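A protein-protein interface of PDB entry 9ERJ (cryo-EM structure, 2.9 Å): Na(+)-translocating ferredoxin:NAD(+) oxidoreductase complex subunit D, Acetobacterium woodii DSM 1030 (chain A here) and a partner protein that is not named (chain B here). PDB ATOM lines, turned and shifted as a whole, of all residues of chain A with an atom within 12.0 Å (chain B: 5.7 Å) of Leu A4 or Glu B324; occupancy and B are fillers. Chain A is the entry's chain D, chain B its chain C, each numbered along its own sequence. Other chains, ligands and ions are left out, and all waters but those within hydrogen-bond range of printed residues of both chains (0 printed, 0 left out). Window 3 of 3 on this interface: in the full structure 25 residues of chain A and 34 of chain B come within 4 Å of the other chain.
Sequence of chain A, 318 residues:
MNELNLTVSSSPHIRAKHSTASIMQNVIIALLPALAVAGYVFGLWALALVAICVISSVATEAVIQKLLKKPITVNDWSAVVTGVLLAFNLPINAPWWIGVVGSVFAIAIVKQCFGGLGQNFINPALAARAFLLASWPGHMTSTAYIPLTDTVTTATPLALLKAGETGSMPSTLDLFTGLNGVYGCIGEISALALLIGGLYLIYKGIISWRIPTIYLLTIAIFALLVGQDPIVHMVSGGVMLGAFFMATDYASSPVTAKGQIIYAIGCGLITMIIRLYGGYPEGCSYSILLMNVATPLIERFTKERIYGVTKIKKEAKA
The backbone carbonyl oxygen (O) of Gly B326 lies within hydrogen-bond range of the side-chain hydroxyl (OG1) of Thr A7 (3.4 Å).
Glu B324 touches Leu A4 (OE2 to CD2, 3.6 Å). Leu A6 touches Pro B325 (CD2 to O, 3.9 Å). Val B328 touches Leu A6. O of Phe B340 touches CD1 of Leu A6 (3.98 Å). CE2 of Phe B340 touches CG1 of Val A8 (3.7 Å).
Of the 13 printed residues of chain B, 5 touch a printed residue of chain A. Printed residues of chain B that touch a printed residue of chain A: Glu B324, Pro B325, Gly B326, Val B328 and Phe B340. Hydrophobic or aromatic side chains of chain B within 4 Å of the printed part of chain A: Val B328 and Phe B340. Among the printed residues, 6 pairs touch across the chains. Among the printed residues, no Asp or Glu carboxylate lies within 4 Å of a Lys or Arg side-chain nitrogen of the other chain.
The backbone carbonyl oxygen (O) of Leu B356 is in hydrogen-bond range of the backbone NH (N) of Gly B326, at 2.8 Å.
Of chain B, only Glu B324 comes within 4 Å of Leu A4. Glu B324 touches just one residue of chain A: Leu A4 (3.6 Å). No residue of chain A comes within 4 Å of Ala B296. No residue of chain A comes within 4 Å of Phe B321. No residue of chain A comes within 4 Å of Ser B322. Pro B325 touches one residue of chain A. Gly B326 touches just one residue of chain A: Thr A7. No residue of chain A comes within 4 Å of Thr B357. Lys B358 touches none of the printed residues of chain A. Printed residues of chain B within 4 Å of Leu A6: Pro B325 (3.9 Å), Val B328 (3.9 Å) and Phe B340 (3.98 Å). Printed residues of chain B within 4 Å of Val A8: Phe B340 (3.7 Å). Printed residues of chain A within 4 Å of Phe B340: Leu A6 and Val A8. Printed residues of chain B within 4 Å of Thr A7: Gly B326 (3.4 Å). The nearest printed residue of chain A that does not touch Val B328 is Thr A7 (5.5 Å).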
ATOM      1  N   MET A   1       5.792   1.941  -4.623  1.00  0.00           N
ATOM      2  CA  MET A   1       6.619   3.140  -4.700  1.00  0.00           C
ATOM      3  C   MET A   1       7.304   3.242  -6.059  1.00  0.00           C
ATOM      4  O   MET A   1       8.446   3.688  -6.156  1.00  0.00           O
ATOM      5  CB  MET A   1       7.664   3.143  -3.583  1.00  0.00           C
ATOM      6  CG  MET A   1       7.131   2.691  -2.232  1.00  0.00           C
ATOM      7  SD  MET A   1       7.717   3.714  -0.869  1.00  0.00           S
ATOM      8  CE  MET A   1       6.407   4.932  -0.770  1.00  0.00           C
ATOM      9  N   ASN A   2       6.597   2.823  -7.105  1.00  0.00           N
ATOM     10  CA  ASN A   2       7.152   2.841  -8.451  1.00  0.00           C
ATOM     11  C   ASN A   2       6.922   4.199  -9.104  1.00  0.00           C
ATOM     12  O   ASN A   2       5.789   4.687  -9.164  1.00  0.00           O
ATOM     13  CB  ASN A   2       6.531   1.730  -9.299  1.00  0.00           C
ATOM     14  CG  ASN A   2       5.021   1.664  -9.161  1.00  0.00           C
ATOM     15  OD1 ASN A   2       4.438   2.289  -8.275  1.00  0.00           O
ATOM     16  ND2 ASN A   2       4.379   0.905 -10.042  1.00  0.00           N
ATOM     17  N   GLU A   3       8.000   4.808  -9.589  1.00  0.00           N
ATOM     18  CA  GLU A   3       7.916   6.070 -10.302  1.00  0.00           C
ATOM     19  C   GLU A   3       7.654   5.807 -11.785  1.00  0.00           C
ATOM     20  O   GLU A   3       7.607   4.662 -12.241  1.00  0.00           O
ATOM     21  CB  GLU A   3       9.192   6.885 -10.096  1.00  0.00           C
ATOM     22  CG  GLU A   3       8.965   8.387  -9.973  1.00  0.00           C
ATOM     23  CD  GLU A   3      10.225   9.191 -10.236  1.00  0.00           C
ATOM     24  OE1 GLU A   3      11.227   8.598 -10.688  1.00  0.00           O
ATOM     25  OE2 GLU A   3      10.212  10.416  -9.996  1.00  0.00           O
ATOM     26  N   LEU A   4       7.478   6.880 -12.549  1.00  0.00           N
ATOM     27  CA  LEU A   4       7.236   6.786 -13.984  1.00  0.00           C
ATOM     28  C   LEU A   4       8.396   7.290 -14.826  1.00  0.00           C
ATOM     29  O   LEU A   4       8.792   6.614 -15.779  1.00  0.00           O
ATOM     30  CB  LEU A   4       5.966   7.559 -14.356  1.00  0.00           C
ATOM     31  CG  LEU A   4       4.651   6.775 -14.318  1.00  0.00           C
ATOM     32  CD1 LEU A   4       3.495   7.638 -14.795  1.00  0.00           C
ATOM     33  CD2 LEU A   4       4.753   5.509 -15.151  1.00  0.00           C
ATOM     34  N   ASN A   5       8.950   8.454 -14.487  1.00  0.00           N
ATOM     35  CA  ASN A   5      10.070   9.072 -15.201  1.00  0.00           C
ATOM     36  C   ASN A   5       9.755   9.242 -16.688  1.00  0.00           C
ATOM     37  O   ASN A   5      10.374   8.635 -17.563  1.00  0.00           O
ATOM     38  CB  ASN A   5      11.364   8.280 -14.998  1.00  0.00           C
ATOM     39  CG  ASN A   5      12.599   9.161 -15.041  1.00  0.00           C
ATOM     40  OD1 ASN A   5      13.470   8.986 -15.891  1.00  0.00           O
ATOM     41  ND2 ASN A   5      12.676  10.118 -14.123  1.00  0.00           N
ATOM     42  N   LEU A   6       8.763  10.083 -16.958  1.00  0.00           N
ATOM     43  CA  LEU A   6       8.349  10.359 -18.321  1.00  0.00           C
ATOM     44  C   LEU A   6       9.306  11.353 -18.978  1.00  0.00           C
ATOM     45  O   LEU A   6      10.242  11.861 -18.359  1.00  0.00           O
ATOM     46  CB  LEU A   6       6.916  10.888 -18.341  1.00  0.00           C
ATOM     47  CG  LEU A   6       5.900  10.036 -17.578  1.00  0.00           C
ATOM     48  CD1 LEU A   6       4.531  10.685 -17.590  1.00  0.00           C
ATOM     49  CD2 LEU A   6       5.833   8.638 -18.163  1.00  0.00           C
ATOM     50  N   THR A   7       9.066  11.619 -20.258  1.00  0.00           N
ATOM     51  CA  THR A   7       9.873  12.553 -21.030  1.00  0.00           C
ATOM     52  C   THR A   7       9.058  13.798 -21.351  1.00  0.00           C
ATOM     53  O   THR A   7       7.886  13.704 -21.726  1.00  0.00           O
ATOM     54  CB  THR A   7      10.369  11.907 -22.325  1.00  0.00           C
ATOM     55  OG1 THR A   7      10.894  10.605 -22.040  1.00  0.00           O
ATOM     56  CG2 THR A   7      11.458  12.750 -22.965  1.00  0.00           C
ATOM     57  N   VAL A   8       9.681  14.963 -21.199  1.00  0.00           N
ATOM     58  CA  VAL A   8       9.045  16.245 -21.479  1.00  0.00           C
ATOM     59  C   VAL A   8       9.805  16.924 -22.608  1.00  0.00           C
ATOM     60  O   VAL A   8      11.041  16.957 -22.602  1.00  0.00           O
ATOM     61  CB  VAL A   8       8.988  17.144 -20.228  1.00  0.00           C
ATOM     62  CG1 VAL A   8       7.870  16.693 -19.309  1.00  0.00           C
ATOM     63  CG2 VAL A   8      10.314  17.132 -19.489  1.00  0.00           C
ATOM     64  N   ALA B 296       0.348   2.331 -25.462  1.00  0.00           N
ATOM     65  CA  ALA B 296       0.457   1.654 -24.176  1.00  0.00           C
ATOM     66  C   ALA B 296      -0.891   1.514 -23.477  1.00  0.00           C
ATOM     67  O   ALA B 296      -0.941   1.399 -22.248  1.00  0.00           O
ATOM     68  CB  ALA B 296       1.450   2.386 -23.276  1.00  0.00           C
ATOM     69  N   PHE B 321      -2.199  -0.020 -18.440  1.00  0.00           N
ATOM     70  CA  PHE B 321      -0.956   0.013 -19.201  1.00  0.00           C
ATOM     71  C   PHE B 321      -0.548  -1.409 -19.566  1.00  0.00           C
ATOM     72  O   PHE B 321      -0.352  -2.250 -18.682  1.00  0.00           O
ATOM     73  CB  PHE B 321       0.153   0.695 -18.400  1.00  0.00           C
ATOM     74  CG  PHE B 321       0.014   2.186 -18.311  1.00  0.00           C
ATOM     75  CD1 PHE B 321      -0.191   2.947 -19.448  1.00  0.00           C
ATOM     76  CD2 PHE B 321       0.098   2.830 -17.087  1.00  0.00           C
ATOM     77  CE1 PHE B 321      -0.315   4.321 -19.366  1.00  0.00           C
ATOM     78  CE2 PHE B 321      -0.026   4.202 -17.001  1.00  0.00           C
ATOM     79  CZ  PHE B 321      -0.232   4.947 -18.141  1.00  0.00           C
ATOM     80  N   SER B 322      -0.426  -1.677 -20.868  1.00  0.00           N
ATOM     81  CA  SER B 322       0.090  -2.972 -21.301  1.00  0.00           C
ATOM     82  C   SER B 322       1.599  -3.061 -21.109  1.00  0.00           C
ATOM     83  O   SER B 322       2.131  -4.153 -20.881  1.00  0.00           O
ATOM     84  CB  SER B 322      -0.277  -3.227 -22.762  1.00  0.00           C
ATOM     85  OG  SER B 322       0.169  -2.170 -23.593  1.00  0.00           O
ATOM     86  N   SER B 323       2.297  -1.931 -21.196  1.00  0.00           N
ATOM     87  CA  SER B 323       3.734  -1.867 -20.977  1.00  0.00           C
ATOM     88  C   SER B 323       4.052  -0.557 -20.268  1.00  0.00           C
ATOM     89  O   SER B 323       3.161   0.240 -19.962  1.00  0.00           O
ATOM     90  CB  SER B 323       4.505  -1.993 -22.295  1.00  0.00           C
ATOM     91  OG  SER B 323       4.252  -0.887 -23.142  1.00  0.00           O
ATOM     92  N   GLU B 324       5.331  -0.337 -20.001  1.00  0.00           N
ATOM     93  CA  GLU B 324       5.752   0.883 -19.323  1.00  0.00           C
ATOM     94  C   GLU B 324       5.698   2.058 -20.291  1.00  0.00           C
ATOM     95  O   GLU B 324       6.377   2.025 -21.327  1.00  0.00           O
ATOM     96  CB  GLU B 324       7.162   0.718 -18.764  1.00  0.00           C
ATOM     97  CG  GLU B 324       7.224   0.643 -17.248  1.00  0.00           C
ATOM     98  CD  GLU B 324       7.035   1.993 -16.587  1.00  0.00           C
ATOM     99  OE1 GLU B 324       7.948   2.840 -16.685  1.00  0.00           O
ATOM    100  OE2 GLU B 324       5.971   2.209 -15.968  1.00  0.00           O
ATOM    101  N   PRO B 325       4.920   3.098 -20.010  1.00  0.00           N
ATOM    102  CA  PRO B 325       4.849   4.238 -20.925  1.00  0.00           C
ATOM    103  C   PRO B 325       6.087   5.115 -20.842  1.00  0.00           C
ATOM    104  O   PRO B 325       6.765   5.188 -19.815  1.00  0.00           O
ATOM    105  CB  PRO B 325       3.606   4.994 -20.444  1.00  0.00           C
ATOM    106  CG  PRO B 325       3.540   4.692 -18.992  1.00  0.00           C
ATOM    107  CD  PRO B 325       4.080   3.294 -18.815  1.00  0.00           C
ATOM    108  N   GLY B 326       6.373   5.789 -21.951  1.00  0.00           N
ATOM    109  CA  GLY B 326       7.500   6.697 -22.005  1.00  0.00           C
ATOM    110  C   GLY B 326       7.089   8.140 -22.203  1.00  0.00           C
ATOM    111  O   GLY B 326       7.926   9.043 -22.128  1.00  0.00           O
ATOM    112  N   VAL B 328       3.249  10.719 -21.825  1.00  0.00           N
ATOM    113  CA  VAL B 328       1.813  10.923 -21.652  1.00  0.00           C
ATOM    114  C   VAL B 328       1.487  12.333 -22.125  1.00  0.00           C
ATOM    115  O   VAL B 328       2.084  13.305 -21.649  1.00  0.00           O
ATOM    116  CB  VAL B 328       1.376  10.717 -20.192  1.00  0.00           C
ATOM    117  CG1 VAL B 328      -0.090  11.076 -20.019  1.00  0.00           C
ATOM    118  CG2 VAL B 328       1.628   9.282 -19.761  1.00  0.00           C
ATOM    119  N   PHE B 340       3.772  15.574 -16.440  1.00  0.00           N
ATOM    120  CA  PHE B 340       4.720  15.103 -15.438  1.00  0.00           C
ATOM    121  C   PHE B 340       4.154  13.967 -14.594  1.00  0.00           C
ATOM    122  O   PHE B 340       4.843  12.974 -14.347  1.00  0.00           O
ATOM    123  CB  PHE B 340       5.146  16.256 -14.520  1.00  0.00           C
ATOM    124  CG  PHE B 340       5.933  17.334 -15.212  1.00  0.00           C
ATOM    125  CD1 PHE B 340       5.293  18.424 -15.777  1.00  0.00           C
ATOM    126  CD2 PHE B 340       7.314  17.265 -15.283  1.00  0.00           C
ATOM    127  CE1 PHE B 340       6.013  19.420 -16.408  1.00  0.00           C
ATOM    128  CE2 PHE B 340       8.038  18.258 -15.912  1.00  0.00           C
ATOM    129  CZ  PHE B 340       7.386  19.336 -16.474  1.00  0.00           C
ATOM    130  N   THR B 342       0.188  11.842 -13.271  1.00  0.00           N
ATOM    131  CA  THR B 342      -1.141  11.426 -13.701  1.00  0.00           C
ATOM    132  C   THR B 342      -2.225  11.812 -12.699  1.00  0.00           C
ATOM    133  O   THR B 342      -3.318  11.240 -12.723  1.00  0.00           O
ATOM    134  CB  THR B 342      -1.175   9.918 -13.956  1.00  0.00           C
ATOM    135  OG1 THR B 342      -0.945   9.218 -12.727  1.00  0.00           O
ATOM    136  CG2 THR B 342      -0.112   9.523 -14.967  1.00  0.00           C
ATOM    137  N   LEU B 356       2.288   6.918 -25.126  1.00  0.00           N
ATOM    138  CA  LEU B 356       3.253   6.307 -26.026  1.00  0.00           C
ATOM    139  C   LEU B 356       4.199   5.402 -25.248  1.00  0.00           C
ATOM    140  O   LEU B 356       4.520   5.654 -24.084  1.00  0.00           O
ATOM    141  CB  LEU B 356       4.055   7.377 -26.777  1.00  0.00           C
ATOM    142  CG  LEU B 356       3.612   7.741 -28.194  1.00  0.00           C
ATOM    143  CD1 LEU B 356       2.243   8.375 -28.184  1.00  0.00           C
ATOM    144  CD2 LEU B 356       4.619   8.681 -28.828  1.00  0.00           C
ATOM    145  N   THR B 357       4.645   4.338 -25.909  1.00  0.00           N
ATOM    146  CA  THR B 357       5.584   3.409 -25.306  1.00  0.00           C
ATOM    147  C   THR B 357       7.001   3.973 -25.402  1.00  0.00           C
ATOM    148  O   THR B 357       7.240   5.024 -25.999  1.00  0.00           O
ATOM    149  CB  THR B 357       5.478   2.036 -25.969  1.00  0.00           C
ATOM    150  OG1 THR B 357       6.204   1.073 -25.195  1.00  0.00           O
ATOM    151  CG2 THR B 357       6.046   2.076 -27.374  1.00  0.00           C
ATOM    152  N   LYS B 358       7.958   3.269 -24.793  1.00  0.00           N
ATOM    153  CA  LYS B 358       9.325   3.777 -24.734  1.00  0.00           C
ATOM    154  C   LYS B 358       9.999   3.742 -26.099  1.00  0.00           C
ATOM    155  O   LYS B 358      10.786   4.635 -26.431  1.00  0.00           O
ATOM    156  CB  LYS B 358      10.137   2.980 -23.714  1.00  0.00           C
ATOM    157  CG  LYS B 358      10.195   3.621 -22.338  1.00  0.00           C
ATOM    158  CD  LYS B 358      10.947   2.747 -21.351  1.00  0.00           C
ATOM    159  CE  LYS B 358      10.422   2.939 -19.940  1.00  0.00           C
ATOM    160  NZ  LYS B 358      10.452   4.369 -19.530  1.00  0.00           N
